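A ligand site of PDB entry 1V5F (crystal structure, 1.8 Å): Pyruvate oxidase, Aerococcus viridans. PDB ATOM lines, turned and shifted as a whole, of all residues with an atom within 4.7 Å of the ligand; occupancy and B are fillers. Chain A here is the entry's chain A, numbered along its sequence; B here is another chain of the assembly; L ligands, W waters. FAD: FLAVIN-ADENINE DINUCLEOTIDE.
O4B of the ligand sits close to O of Gly 276 (3.1 Å). CA of Gly 212 touches O2P of the ligand, 3.0 Å away. CA of Gly 214 touches C4A of the ligand (3.4 Å). Tyr 255 touches the ligand. Phe 279 touches the ligand. Pro 280 touches the ligand. Phe 281 touches the ligand (CE2 to C4X, 3.6 Å). CB of Asp 300 touches O2B of the ligand, at 3.6 Å. O of Gly 316 touches C2A of the ligand, at 3.6 Å. Gln 391 touches the ligand. Ser 408 touches the ligand. Ala 412 touches the ligand. Phe 113 of chain B touches the ligand (CE1 to C8, 3.4 Å). Of the 35 residues printed, 28 come within 4 Å of the ligand.
O2P of the ligand is in hydrogen-bond range of OG1 of Thr 236, 2.6 Å away. O of Val 257 lies close to N3 of the ligand (3.5 Å). The backbone carbonyl oxygen (O) of Pro 409 sits at hydrogen-bond distance from an oxygen (O2') of the ligand, 2.7 Å away. The backbone NH (N) of Arg 256 is in hydrogen-bond range of an oxygen (O4) of the ligand (3.4 Å). N of Gly 237 lies within hydrogen-bond range of O2 of the ligand, 3.2 Å away. O1P of the ligand is in hydrogen-bond range of N of Asn 278 (2.9 Å). The backbone carbonyl oxygen (O) of Thr 254 sits at hydrogen-bond distance from a nitrogen (N3) of the ligand (2.9 Å). The backbone NH (N) of Ile 213 lies within hydrogen-bond range of an oxygen (O2P) of the ligand (2.8 Å). SD of Met 303 lies close to O3B of the ligand. NZ of Lys 238 is in salt-bridge range of O1A of the ligand (2.6 Å). The side-chain carboxylate (OD2) of Asp 298 lies within hydrogen-bond range of an oxygen (O3B) of the ligand, at 2.7 Å. N6A of the ligand sits at hydrogen-bond distance from OD1 of Asp 317, at 2.9 Å. A nitrogen (N3A) of the ligand lies within hydrogen-bond range of the backbone NH (N) of Ile 299 (3.5 Å). The backbone NH (N) of Val 257 lies within hydrogen-bond range of an oxygen (O4) of the ligand (2.6 Å). An oxygen (O1P) of the ligand lies within hydrogen-bond range of the side-chain hydroxyl of Ser 277. N of Ala 318 is in hydrogen-bond range of N1A of the ligand, at 2.9 Å.
N of Gly 316 lies within hydrogen-bond range of O of Asp 298 (2.9 Å). The backbone carbonyl oxygen (O) of Gly 276 is in hydrogen-bond range of the backbone NH (N) of Ile 213 (3.3 Å). OH of Tyr 255 sits at hydrogen-bond distance from NE of Arg 256 (3.3 Å). The backbone NH (N) of Gly 276 is in hydrogen-bond range of the backbone carbonyl oxygen (O) of Ile 297 (2.9 Å). The backbone NH of Gly 212 lies close to the backbone carbonyl oxygen of Gly 276, at 3.5 Å. O of Val 257 lies within hydrogen-bond range of OG of Ser 253. The backbone NH (N) of Asn 239 lies close to the side-chain hydroxyl (OG1) of Thr 236 (3.4 Å). OG of Ser 408 lies within hydrogen-bond range of N of Ala 412, at 3.1 Å.
Water W10 bridges an oxygen (O2B) of the ligand (2.7 Å) and the side-chain carboxylate of Asp 300 (2.8 Å). Water W6 lies within hydrogen-bond range of O2 of the ligand (2.7 Å), O of Thr 235 (2.8 Å) and N of Thr 254 (3.1 Å). Water W8 bridges ND2 of Asn 278 (2.9 Å) and O2A of the ligand (3.0 Å). Water W3 lies within hydrogen-bond range of the side-chain amide oxygen (OE1) of Gln 391 (2.9 Å) and the backbone carbonyl oxygen (O) of Gly 237 (3.2 Å).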
ATOM      1  N   GLY A 212      24.813 -26.138 -30.672  1.00  0.00           N
ATOM      2  CA  GLY A 212      25.078 -27.154 -29.669  1.00  0.00           C
ATOM      3  C   GLY A 212      24.410 -28.456 -30.094  1.00  0.00           C
ATOM      4  O   GLY A 212      23.850 -28.520 -31.187  1.00  0.00           O
ATOM      5  N   ILE A 213      24.440 -29.479 -29.242  1.00  0.00           N
ATOM      6  CA  ILE A 213      23.868 -30.769 -29.614  1.00  0.00           C
ATOM      7  C   ILE A 213      22.373 -30.761 -29.908  1.00  0.00           C
ATOM      8  O   ILE A 213      21.833 -31.779 -30.349  1.00  0.00           O
ATOM      9  CB  ILE A 213      24.163 -31.868 -28.581  1.00  0.00           C
ATOM     10  CG1 ILE A 213      23.519 -31.537 -27.227  1.00  0.00           C
ATOM     11  CG2 ILE A 213      25.663 -32.057 -28.452  1.00  0.00           C
ATOM     12  CD1 ILE A 213      23.529 -32.715 -26.261  1.00  0.00           C
ATOM     13  N   GLY A 214      21.714 -29.632 -29.662  1.00  0.00           N
ATOM     14  CA  GLY A 214      20.308 -29.551 -29.981  1.00  0.00           C
ATOM     15  C   GLY A 214      20.136 -29.670 -31.479  1.00  0.00           C
ATOM     16  O   GLY A 214      19.063 -30.008 -31.987  1.00  0.00           O
ATOM     17  N   THR A 235      30.773 -24.262 -33.053  1.00  0.00           N
ATOM     18  CA  THR A 235      30.144 -25.424 -32.455  1.00  0.00           C
ATOM     19  C   THR A 235      30.577 -25.556 -31.005  1.00  0.00           C
ATOM     20  O   THR A 235      31.458 -24.826 -30.556  1.00  0.00           O
ATOM     21  CB  THR A 235      30.501 -26.719 -33.226  1.00  0.00           C
ATOM     22  OG1 THR A 235      29.846 -27.829 -32.617  1.00  0.00           O
ATOM     23  CG2 THR A 235      32.013 -26.955 -33.201  1.00  0.00           C
ATOM     24  N   THR A 236      29.952 -26.466 -30.281  1.00  0.00           N
ATOM     25  CA  THR A 236      30.301 -26.698 -28.880  1.00  0.00           C
ATOM     26  C   THR A 236      31.205 -27.917 -28.811  1.00  0.00           C
ATOM     27  O   THR A 236      31.278 -28.695 -29.769  1.00  0.00           O
ATOM     28  CB  THR A 236      29.048 -26.983 -28.033  1.00  0.00           C
ATOM     29  OG1 THR A 236      28.413 -28.173 -28.505  1.00  0.00           O
ATOM     30  CG2 THR A 236      28.069 -25.831 -28.128  1.00  0.00           C
ATOM     31  N   GLY A 237      31.903 -28.080 -27.687  1.00  0.00           N
ATOM     32  CA  GLY A 237      32.798 -29.210 -27.533  1.00  0.00           C
ATOM     33  C   GLY A 237      32.118 -30.570 -27.631  1.00  0.00           C
ATOM     34  O   GLY A 237      32.796 -31.581 -27.801  1.00  0.00           O
ATOM     35  N   LYS A 238      30.798 -30.607 -27.510  1.00  0.00           N
ATOM     36  CA  LYS A 238      30.048 -31.866 -27.590  1.00  0.00           C
ATOM     37  C   LYS A 238      29.439 -32.111 -28.979  1.00  0.00           C
ATOM     38  O   LYS A 238      28.998 -33.220 -29.269  1.00  0.00           O
ATOM     39  CB  LYS A 238      28.882 -31.862 -26.589  1.00  0.00           C
ATOM     40  CG  LYS A 238      29.245 -32.010 -25.126  1.00  0.00           C
ATOM     41  CD  LYS A 238      28.021 -31.835 -24.206  1.00  0.00           C
ATOM     42  CE  LYS A 238      26.947 -32.889 -24.463  1.00  0.00           C
ATOM     43  NZ  LYS A 238      25.819 -32.783 -23.489  1.00  0.00           N
ATOM     44  N   ASN A 239      29.446 -31.085 -29.817  1.00  0.00           N
ATOM     45  CA  ASN A 239      28.776 -31.154 -31.125  1.00  0.00           C
ATOM     46  C   ASN A 239      29.573 -31.159 -32.434  1.00  0.00           C
ATOM     47  O   ASN A 239      29.017 -30.869 -33.489  1.00  0.00           O
ATOM     48  CB  ASN A 239      27.759 -30.006 -31.167  1.00  0.00           C
ATOM     49  CG  ASN A 239      26.673 -30.223 -32.198  1.00  0.00           C
ATOM     50  OD1 ASN A 239      26.104 -31.310 -32.303  1.00  0.00           O
ATOM     51  ND2 ASN A 239      26.366 -29.165 -32.945  1.00  0.00           N
ATOM     52  N   SER A 253      35.238 -24.468 -31.914  1.00  0.00           N
ATOM     53  CA  SER A 253      34.575 -24.141 -30.653  1.00  0.00           C
ATOM     54  C   SER A 253      35.320 -23.020 -29.929  1.00  0.00           C
ATOM     55  O   SER A 253      36.495 -22.783 -30.195  1.00  0.00           O
ATOM     56  CB  SER A 253      34.502 -25.389 -29.767  1.00  0.00           C
ATOM     57  OG  SER A 253      35.767 -26.018 -29.668  1.00  0.00           O
ATOM     58  N   THR A 254      34.638 -22.328 -29.005  1.00  0.00           N
ATOM     59  CA  THR A 254      35.285 -21.243 -28.269  1.00  0.00           C
ATOM     60  C   THR A 254      35.901 -21.698 -26.938  1.00  0.00           C
ATOM     61  O   THR A 254      35.640 -22.810 -26.457  1.00  0.00           O
ATOM     62  CB  THR A 254      34.316 -20.069 -27.979  1.00  0.00           C
ATOM     63  OG1 THR A 254      33.364 -20.446 -26.985  1.00  0.00           O
ATOM     64  CG2 THR A 254      33.596 -19.652 -29.261  1.00  0.00           C
ATOM     65  N   TYR A 255      36.712 -20.816 -26.374  1.00  0.00           N
ATOM     66  CA  TYR A 255      37.446 -21.038 -25.128  1.00  0.00           C
ATOM     67  C   TYR A 255      38.615 -22.021 -25.325  1.00  0.00           C
ATOM     68  O   TYR A 255      39.043 -22.251 -26.461  1.00  0.00           O
ATOM     69  CB  TYR A 255      36.517 -21.497 -23.987  1.00  0.00           C
ATOM     70  CG  TYR A 255      37.153 -21.329 -22.623  1.00  0.00           C
ATOM     71  CD1 TYR A 255      37.796 -20.139 -22.269  1.00  0.00           C
ATOM     72  CD2 TYR A 255      37.189 -22.379 -21.710  1.00  0.00           C
ATOM     73  CE1 TYR A 255      38.467 -20.004 -21.054  1.00  0.00           C
ATOM     74  CE2 TYR A 255      37.860 -22.254 -20.485  1.00  0.00           C
ATOM     75  CZ  TYR A 255      38.492 -21.064 -20.170  1.00  0.00           C
ATOM     76  OH  TYR A 255      39.183 -20.946 -18.991  1.00  0.00           O
ATOM     77  N   ARG A 256      39.118 -22.601 -24.238  1.00  0.00           N
ATOM     78  CA  ARG A 256      40.273 -23.505 -24.280  1.00  0.00           C
ATOM     79  C   ARG A 256      40.236 -24.725 -25.197  1.00  0.00           C
ATOM     80  O   ARG A 256      41.137 -24.909 -26.016  1.00  0.00           O
ATOM     81  CB  ARG A 256      40.608 -23.958 -22.857  1.00  0.00           C
ATOM     82  CG  ARG A 256      41.090 -22.835 -21.972  1.00  0.00           C
ATOM     83  CD  ARG A 256      41.489 -23.345 -20.603  1.00  0.00           C
ATOM     84  NE  ARG A 256      42.054 -22.280 -19.781  1.00  0.00           N
ATOM     85  CZ  ARG A 256      42.374 -22.422 -18.500  1.00  0.00           C
ATOM     86  NH1 ARG A 256      42.887 -21.398 -17.827  1.00  0.00           N
ATOM     87  NH2 ARG A 256      42.183 -23.589 -17.893  1.00  0.00           N
ATOM     88  N   VAL A 257      39.226 -25.576 -25.048  1.00  0.00           N
ATOM     89  CA  VAL A 257      39.133 -26.735 -25.926  1.00  0.00           C
ATOM     90  C   VAL A 257      38.358 -26.253 -27.147  1.00  0.00           C
ATOM     91  O   VAL A 257      37.165 -26.525 -27.309  1.00  0.00           O
ATOM     92  CB  VAL A 257      38.386 -27.908 -25.244  1.00  0.00           C
ATOM     93  CG1 VAL A 257      38.188 -29.057 -26.215  1.00  0.00           C
ATOM     94  CG2 VAL A 257      39.189 -28.374 -24.037  1.00  0.00           C
ATOM     95  N   GLY A 258      39.059 -25.512 -28.003  1.00  0.00           N
ATOM     96  CA  GLY A 258      38.449 -24.970 -29.200  1.00  0.00           C
ATOM     97  C   GLY A 258      39.492 -24.666 -30.252  1.00  0.00           C
ATOM     98  O   GLY A 258      40.608 -25.194 -30.198  1.00  0.00           O
ATOM     99  N   GLY A 276      20.211 -24.737 -29.792  1.00  0.00           N
ATOM    100  CA  GLY A 276      20.364 -25.973 -29.035  1.00  0.00           C
ATOM    101  C   GLY A 276      21.644 -26.103 -28.235  1.00  0.00           C
ATOM    102  O   GLY A 276      22.372 -27.090 -28.372  1.00  0.00           O
ATOM    103  N   SER A 277      21.914 -25.120 -27.383  1.00  0.00           N
ATOM    104  CA  SER A 277      23.123 -25.148 -26.566  1.00  0.00           C
ATOM    105  C   SER A 277      22.918 -24.605 -25.151  1.00  0.00           C
ATOM    106  O   SER A 277      22.013 -23.810 -24.892  1.00  0.00           O
ATOM    107  CB  SER A 277      24.239 -24.337 -27.243  1.00  0.00           C
ATOM    108  OG  SER A 277      25.385 -24.233 -26.408  1.00  0.00           O
ATOM    109  N   ASN A 278      23.775 -25.057 -24.243  1.00  0.00           N
ATOM    110  CA  ASN A 278      23.757 -24.591 -22.857  1.00  0.00           C
ATOM    111  C   ASN A 278      25.225 -24.425 -22.445  1.00  0.00           C
ATOM    112  O   ASN A 278      25.620 -24.775 -21.324  1.00  0.00           O
ATOM    113  CB  ASN A 278      23.037 -25.592 -21.948  1.00  0.00           C
ATOM    114  CG  ASN A 278      22.772 -25.018 -20.554  1.00  0.00           C
ATOM    115  OD1 ASN A 278      22.482 -23.827 -20.414  1.00  0.00           O
ATOM    116  ND2 ASN A 278      22.839 -25.859 -19.535  1.00  0.00           N
ATOM    117  N   PHE A 279      26.012 -23.899 -23.387  1.00  0.00           N
ATOM    118  CA  PHE A 279      27.448 -23.637 -23.218  1.00  0.00           C
ATOM    119  C   PHE A 279      27.701 -23.124 -21.797  1.00  0.00           C
ATOM    120  O   PHE A 279      27.322 -22.002 -21.462  1.00  0.00           O
ATOM    121  CB  PHE A 279      27.871 -22.618 -24.275  1.00  0.00           C
ATOM    122  CG  PHE A 279      29.358 -22.375 -24.329  1.00  0.00           C
ATOM    123  CD1 PHE A 279      30.243 -23.429 -24.535  1.00  0.00           C
ATOM    124  CD2 PHE A 279      29.872 -21.089 -24.200  1.00  0.00           C
ATOM    125  CE1 PHE A 279      31.617 -23.194 -24.610  1.00  0.00           C
ATOM    126  CE2 PHE A 279      31.238 -20.849 -24.271  1.00  0.00           C
ATOM    127  CZ  PHE A 279      32.111 -21.897 -24.481  1.00  0.00           C
ATOM    128  N   PRO A 280      28.371 -23.933 -20.955  1.00  0.00           N
ATOM    129  CA  PRO A 280      28.670 -23.590 -19.561  1.00  0.00           C
ATOM    130  C   PRO A 280      29.656 -22.466 -19.259  1.00  0.00           C
ATOM    131  O   PRO A 280      29.660 -21.917 -18.147  1.00  0.00           O
ATOM    132  CB  PRO A 280      29.133 -24.918 -18.991  1.00  0.00           C
ATOM    133  CG  PRO A 280      29.909 -25.492 -20.153  1.00  0.00           C
ATOM    134  CD  PRO A 280      28.967 -25.230 -21.317  1.00  0.00           C
ATOM    135  N   PHE A 281      30.496 -22.115 -20.232  1.00  0.00           N
ATOM    136  CA  PHE A 281      31.506 -21.071 -20.046  1.00  0.00           C
ATOM    137  C   PHE A 281      30.981 -19.670 -20.380  1.00  0.00           C
ATOM    138  O   PHE A 281      31.644 -18.676 -20.086  1.00  0.00           O
ATOM    139  CB  PHE A 281      32.723 -21.365 -20.934  1.00  0.00           C
ATOM    140  CG  PHE A 281      33.439 -22.650 -20.571  1.00  0.00           C
ATOM    141  CD1 PHE A 281      34.332 -22.690 -19.509  1.00  0.00           C
ATOM    142  CD2 PHE A 281      33.221 -23.817 -21.294  1.00  0.00           C
ATOM    143  CE1 PHE A 281      34.988 -23.872 -19.157  1.00  0.00           C
ATOM    144  CE2 PHE A 281      33.868 -24.997 -20.960  1.00  0.00           C
ATOM    145  CZ  PHE A 281      34.753 -25.031 -19.893  1.00  0.00           C
ATOM    146  N   ILE A 297      17.311 -20.778 -29.583  1.00  0.00           N
ATOM    147  CA  ILE A 297      16.380 -21.849 -29.939  1.00  0.00           C
ATOM    148  C   ILE A 297      16.624 -22.999 -28.978  1.00  0.00           C
ATOM    149  O   ILE A 297      17.767 -23.441 -28.800  1.00  0.00           O
ATOM    150  CB  ILE A 297      16.634 -22.387 -31.368  1.00  0.00           C
ATOM    151  CG1 ILE A 297      16.456 -21.275 -32.403  1.00  0.00           C
ATOM    152  CG2 ILE A 297      15.691 -23.544 -31.651  1.00  0.00           C
ATOM    153  CD1 ILE A 297      16.904 -21.675 -33.801  1.00  0.00           C
ATOM    154  N   ASP A 298      15.571 -23.492 -28.346  1.00  0.00           N
ATOM    155  CA  ASP A 298      15.716 -24.615 -27.420  1.00  0.00           C
ATOM    156  C   ASP A 298      14.367 -25.252 -27.153  1.00  0.00           C
ATOM    157  O   ASP A 298      13.335 -24.594 -27.256  1.00  0.00           O
ATOM    158  CB  ASP A 298      16.341 -24.134 -26.109  1.00  0.00           C
ATOM    159  CG  ASP A 298      17.117 -25.221 -25.385  1.00  0.00           C
ATOM    160  OD1 ASP A 298      16.477 -26.151 -24.838  1.00  0.00           O
ATOM    161  OD2 ASP A 298      18.359 -25.154 -25.380  1.00  0.00           O
ATOM    162  N   ILE A 299      14.359 -26.546 -26.832  1.00  0.00           N
ATOM    163  CA  ILE A 299      13.105 -27.223 -26.541  1.00  0.00           C
ATOM    164  C   ILE A 299      12.796 -27.203 -25.054  1.00  0.00           C
ATOM    165  O   ILE A 299      11.727 -27.627 -24.632  1.00  0.00           O
ATOM    166  CB  ILE A 299      13.128 -28.696 -27.002  1.00  0.00           C
ATOM    167  CG1 ILE A 299      14.336 -29.408 -26.383  1.00  0.00           C
ATOM    168  CG2 ILE A 299      13.130 -28.765 -28.516  1.00  0.00           C
ATOM    169  CD1 ILE A 299      14.345 -30.904 -26.601  1.00  0.00           C
ATOM    170  N   ASP A 300      13.751 -26.704 -24.256  1.00  0.00           N
ATOM    171  CA  ASP A 300      13.591 -26.647 -22.808  1.00  0.00           C
ATOM    172  C   ASP A 300      13.393 -25.210 -22.329  1.00  0.00           C
ATOM    173  O   ASP A 300      14.334 -24.413 -22.335  1.00  0.00           O
ATOM    174  CB  ASP A 300      14.830 -27.263 -22.135  1.00  0.00           C
ATOM    175  CG  ASP A 300      14.718 -27.294 -20.623  1.00  0.00           C
ATOM    176  OD1 ASP A 300      13.698 -26.808 -20.085  1.00  0.00           O
ATOM    177  OD2 ASP A 300      15.657 -27.811 -19.972  1.00  0.00           O
ATOM    178  N   MET A 303      15.948 -23.240 -20.273  1.00  0.00           N
ATOM    179  CA  MET A 303      17.170 -22.739 -20.902  1.00  0.00           C
ATOM    180  C   MET A 303      17.040 -21.392 -21.611  1.00  0.00           C
ATOM    181  O   MET A 303      18.043 -20.746 -21.899  1.00  0.00           O
ATOM    182  CB  MET A 303      17.673 -23.763 -21.928  1.00  0.00           C
ATOM    183  CG  MET A 303      17.945 -25.145 -21.367  1.00  0.00           C
ATOM    184  SD  MET A 303      19.388 -25.162 -20.296  1.00  0.00           S
ATOM    185  CE  MET A 303      18.627 -24.927 -18.654  1.00  0.00           C
ATOM    186  N   GLY A 316      11.201 -24.738 -29.263  1.00  0.00           N
ATOM    187  CA  GLY A 316      10.905 -25.751 -30.254  1.00  0.00           C
ATOM    188  C   GLY A 316      12.117 -26.526 -30.740  1.00  0.00           C
ATOM    189  O   GLY A 316      13.258 -26.188 -30.427  1.00  0.00           O
ATOM    190  N   ASP A 317      11.854 -27.560 -31.523  1.00  0.00           N
ATOM    191  CA  ASP A 317      12.907 -28.393 -32.070  1.00  0.00           C
ATOM    192  C   ASP A 317      13.839 -27.570 -32.968  1.00  0.00           C
ATOM    193  O   ASP A 317      13.375 -26.824 -33.825  1.00  0.00           O
ATOM    194  CB  ASP A 317      12.290 -29.530 -32.875  1.00  0.00           C
ATOM    195  CG  ASP A 317      13.326 -30.452 -33.461  1.00  0.00           C
ATOM    196  OD1 ASP A 317      13.940 -31.230 -32.699  1.00  0.00           O
ATOM    197  OD2 ASP A 317      13.535 -30.397 -34.690  1.00  0.00           O
ATOM    198  N   ALA A 318      15.146 -27.730 -32.768  1.00  0.00           N
ATOM    199  CA  ALA A 318      16.140 -26.993 -33.539  1.00  0.00           C
ATOM    200  C   ALA A 318      16.045 -27.283 -35.034  1.00  0.00           C
ATOM    201  O   ALA A 318      16.292 -26.407 -35.871  1.00  0.00           O
ATOM    202  CB  ALA A 318      17.537 -27.319 -33.034  1.00  0.00           C
ATOM    203  N   VAL A 386      38.803 -37.614 -20.226  1.00  0.00           N
ATOM    204  CA  VAL A 386      39.008 -36.248 -19.763  1.00  0.00           C
ATOM    205  C   VAL A 386      40.486 -35.952 -19.520  1.00  0.00           C
ATOM    206  O   VAL A 386      41.136 -36.616 -18.715  1.00  0.00           O
ATOM    207  CB  VAL A 386      38.217 -35.981 -18.466  1.00  0.00           C
ATOM    208  CG1 VAL A 386      38.503 -34.574 -17.961  1.00  0.00           C
ATOM    209  CG2 VAL A 386      36.731 -36.148 -18.732  1.00  0.00           C
ATOM    210  N   GLN A 391      40.948 -34.262 -25.036  1.00  0.00           N
ATOM    211  CA  GLN A 391      39.989 -33.252 -25.447  1.00  0.00           C
ATOM    212  C   GLN A 391      40.449 -32.467 -26.671  1.00  0.00           C
ATOM    213  O   GLN A 391      39.627 -31.967 -27.443  1.00  0.00           O
ATOM    214  CB  GLN A 391      39.681 -32.297 -24.295  1.00  0.00           C
ATOM    215  CG  GLN A 391      38.877 -32.932 -23.153  1.00  0.00           C
ATOM    216  CD  GLN A 391      37.488 -33.390 -23.580  1.00  0.00           C
ATOM    217  OE1 GLN A 391      36.685 -32.616 -24.095  1.00  0.00           O
ATOM    218  NE2 GLN A 391      37.210 -34.673 -23.354  1.00  0.00           N
ATOM    219  N   SER A 408      32.717 -37.183 -21.049  1.00  0.00           N
ATOM    220  CA  SER A 408      32.050 -36.763 -19.807  1.00  0.00           C
ATOM    221  C   SER A 408      32.362 -35.272 -19.918  1.00  0.00           C
ATOM    222  O   SER A 408      33.353 -34.800 -19.382  1.00  0.00           O
ATOM    223  CB  SER A 408      32.734 -37.366 -18.578  1.00  0.00           C
ATOM    224  OG  SER A 408      32.171 -36.818 -17.395  1.00  0.00           O
ATOM    225  N   PRO A 409      31.509 -34.524 -20.639  1.00  0.00           N
ATOM    226  CA  PRO A 409      31.628 -33.085 -20.895  1.00  0.00           C
ATOM    227  C   PRO A 409      31.359 -32.049 -19.832  1.00  0.00           C
ATOM    228  O   PRO A 409      31.896 -30.939 -19.912  1.00  0.00           O
ATOM    229  CB  PRO A 409      30.703 -32.909 -22.092  1.00  0.00           C
ATOM    230  CG  PRO A 409      29.548 -33.777 -21.698  1.00  0.00           C
ATOM    231  CD  PRO A 409      30.229 -35.039 -21.177  1.00  0.00           C
ATOM    232  N   LEU A 410      30.536 -32.372 -18.841  1.00  0.00           N
ATOM    233  CA  LEU A 410      30.193 -31.393 -17.815  1.00  0.00           C
ATOM    234  C   LEU A 410      30.682 -31.776 -16.418  1.00  0.00           C
ATOM    235  O   LEU A 410      31.320 -30.964 -15.750  1.00  0.00           O
ATOM    236  CB  LEU A 410      28.683 -31.164 -17.807  1.00  0.00           C
ATOM    237  CG  LEU A 410      28.160 -30.016 -16.948  1.00  0.00           C
ATOM    238  CD1 LEU A 410      28.902 -28.729 -17.303  1.00  0.00           C
ATOM    239  CD2 LEU A 410      26.668 -29.862 -17.200  1.00  0.00           C
ATOM    240  N   ALA A 412      32.691 -34.030 -16.156  1.00  0.00           N
ATOM    241  CA  ALA A 412      34.062 -34.245 -16.578  1.00  0.00           C
ATOM    242  C   ALA A 412      34.872 -35.231 -15.755  1.00  0.00           C
ATOM    243  O   ALA A 412      35.984 -34.914 -15.316  1.00  0.00           O
ATOM    244  CB  ALA A 412      34.781 -32.908 -16.630  1.00  0.00           C
ATOM    245  N   PHE B 113      31.494 -24.883 -15.912  1.00  0.00           N
ATOM    246  CA  PHE B 113      32.129 -26.162 -16.166  1.00  0.00           C
ATOM    247  C   PHE B 113      32.511 -26.860 -14.860  1.00  0.00           C
ATOM    248  O   PHE B 113      33.158 -26.254 -13.998  1.00  0.00           O
ATOM    249  CB  PHE B 113      33.372 -25.966 -17.020  1.00  0.00           C
ATOM    250  CG  PHE B 113      34.194 -27.220 -17.176  1.00  0.00           C
ATOM    251  CD1 PHE B 113      33.717 -28.278 -17.929  1.00  0.00           C
ATOM    252  CD2 PHE B 113      35.417 -27.343 -16.539  1.00  0.00           C
ATOM    253  CE1 PHE B 113      34.443 -29.448 -18.045  1.00  0.00           C
ATOM    254  CE2 PHE B 113      36.165 -28.512 -16.643  1.00  0.00           C
ATOM    255  CZ  PHE B 113      35.664 -29.567 -17.395  1.00  0.00           C
HETATM  256  PA  FAD L   1      24.413 -29.253 -23.728  1.00  0.00           P
HETATM  257  O1A FAD L   1      24.181 -30.716 -23.586  1.00  0.00           O
HETATM  258  O2A FAD L   1      25.076 -28.503 -22.627  1.00  0.00           O
HETATM  259  O5B FAD L   1      23.019 -28.528 -23.985  1.00  0.00           O
HETATM  260  C5B FAD L   1      22.288 -28.822 -25.168  1.00  0.00           C
HETATM  261  C4B FAD L   1      21.080 -27.923 -25.270  1.00  0.00           C
HETATM  262  O4B FAD L   1      20.300 -28.312 -26.429  1.00  0.00           O
HETATM  263  C3B FAD L   1      20.128 -27.987 -24.071  1.00  0.00           C
HETATM  264  O3B FAD L   1      19.815 -26.675 -23.618  1.00  0.00           O
HETATM  265  C2B FAD L   1      18.919 -28.763 -24.604  1.00  0.00           C
HETATM  266  O2B FAD L   1      17.705 -28.473 -23.947  1.00  0.00           O
HETATM  267  C1B FAD L   1      18.932 -28.367 -26.081  1.00  0.00           C
HETATM  268  N9A FAD L   1      18.277 -29.325 -26.989  1.00  0.00           N
HETATM  269  C8A FAD L   1      18.296 -30.706 -26.967  1.00  0.00           C
HETATM  270  N7A FAD L   1      17.602 -31.256 -27.944  1.00  0.00           N
HETATM  271  C5A FAD L   1      17.102 -30.174 -28.655  1.00  0.00           C
HETATM  272  C6A FAD L   1      16.287 -30.077 -29.807  1.00  0.00           C
HETATM  273  N6A FAD L   1      15.825 -31.130 -30.476  1.00  0.00           N
HETATM  274  N1A FAD L   1      15.969 -28.825 -30.258  1.00  0.00           N
HETATM  275  C2A FAD L   1      16.433 -27.750 -29.587  1.00  0.00           C
HETATM  276  N3A FAD L   1      17.208 -27.716 -28.487  1.00  0.00           N
HETATM  277  C4A FAD L   1      17.504 -28.972 -28.069  1.00  0.00           C
HETATM  278  N1  FAD L   1      33.203 -27.001 -24.653  1.00  0.00           N
HETATM  279  C2  FAD L   1      33.461 -25.868 -25.380  1.00  0.00           C
HETATM  280  O2  FAD L   1      32.641 -25.417 -26.160  1.00  0.00           O
HETATM  281  N3  FAD L   1      34.693 -25.235 -25.221  1.00  0.00           N
HETATM  282  C4  FAD L   1      35.686 -25.683 -24.383  1.00  0.00           C
HETATM  283  O4  FAD L   1      36.764 -25.063 -24.282  1.00  0.00           O
HETATM  284  C4X FAD L   1      35.418 -26.868 -23.659  1.00  0.00           C
HETATM  285  N5  FAD L   1      36.376 -27.412 -22.817  1.00  0.00           N
HETATM  286  C5X FAD L   1      36.132 -28.583 -22.137  1.00  0.00           C
HETATM  287  C6  FAD L   1      37.120 -29.137 -21.324  1.00  0.00           C
HETATM  288  C7  FAD L   1      36.926 -30.336 -20.640  1.00  0.00           C
HETATM  289  C7M FAD L   1      38.043 -30.899 -19.783  1.00  0.00           C
HETATM  290  C8  FAD L   1      35.661 -30.991 -20.762  1.00  0.00           C
HETATM  291  C8M FAD L   1      35.381 -32.288 -20.047  1.00  0.00           C
HETATM  292  C9  FAD L   1      34.653 -30.436 -21.565  1.00  0.00           C
HETATM  293  C9A FAD L   1      34.867 -29.228 -22.269  1.00  0.00           C
HETATM  294  N10 FAD L   1      33.873 -28.650 -23.099  1.00  0.00           N
HETATM  295  C10 FAD L   1      34.154 -27.494 -23.812  1.00  0.00           C
HETATM  296  C1' FAD L   1      32.498 -29.236 -23.255  1.00  0.00           C
HETATM  297  C2' FAD L   1      31.610 -28.318 -22.384  1.00  0.00           C
HETATM  298  O2' FAD L   1      31.938 -28.476 -21.030  1.00  0.00           O
HETATM  299  C3' FAD L   1      30.103 -28.621 -22.556  1.00  0.00           C
HETATM  300  O3' FAD L   1      29.756 -29.942 -22.163  1.00  0.00           O
HETATM  301  C4' FAD L   1      29.540 -28.500 -23.963  1.00  0.00           C
HETATM  302  O4' FAD L   1      30.073 -27.324 -24.600  1.00  0.00           O
HETATM  303  C5' FAD L   1      28.011 -28.394 -23.917  1.00  0.00           C
HETATM  304  O5' FAD L   1      27.621 -28.413 -25.287  1.00  0.00           O
HETATM  305  P   FAD L   1      26.167 -28.111 -25.856  1.00  0.00           P
HETATM  306  O1P FAD L   1      25.798 -26.715 -25.520  1.00  0.00           O
HETATM  307  O2P FAD L   1      26.148 -28.551 -27.287  1.00  0.00           O
HETATM  308  O3P FAD L   1      25.118 -29.074 -25.167  1.00  0.00           O
HETATM  309  O   HOH W   1      21.785 -31.885 -22.764  1.00  0.00           O
HETATM  310  O   HOH W   2      38.412 -25.701 -21.117  1.00  0.00           O
HETATM  311  O   HOH W   3      34.125 -31.529 -24.894  1.00  0.00           O
HETATM  312  O   HOH W   4      16.637 -33.925 -27.713  1.00  0.00           O
HETATM  313  O   HOH W   5      27.071 -29.461 -21.022  1.00  0.00           O
HETATM  314  O   HOH W   6      31.999 -23.600 -28.092  1.00  0.00           O
HETATM  315  O   HOH W   7      39.952 -30.915 -16.894  1.00  0.00           O
HETATM  316  O   HOH W   8      23.428 -28.635 -20.137  1.00  0.00           O
HETATM  317  O   HOH W   9      19.703 -32.432 -24.559  1.00  0.00           O
HETATM  318  O   HOH W  10      17.797 -29.077 -21.290  1.00  0.00           O
HETATM  319  O   HOH W  11      17.746 -33.958 -30.192  1.00  0.00           O
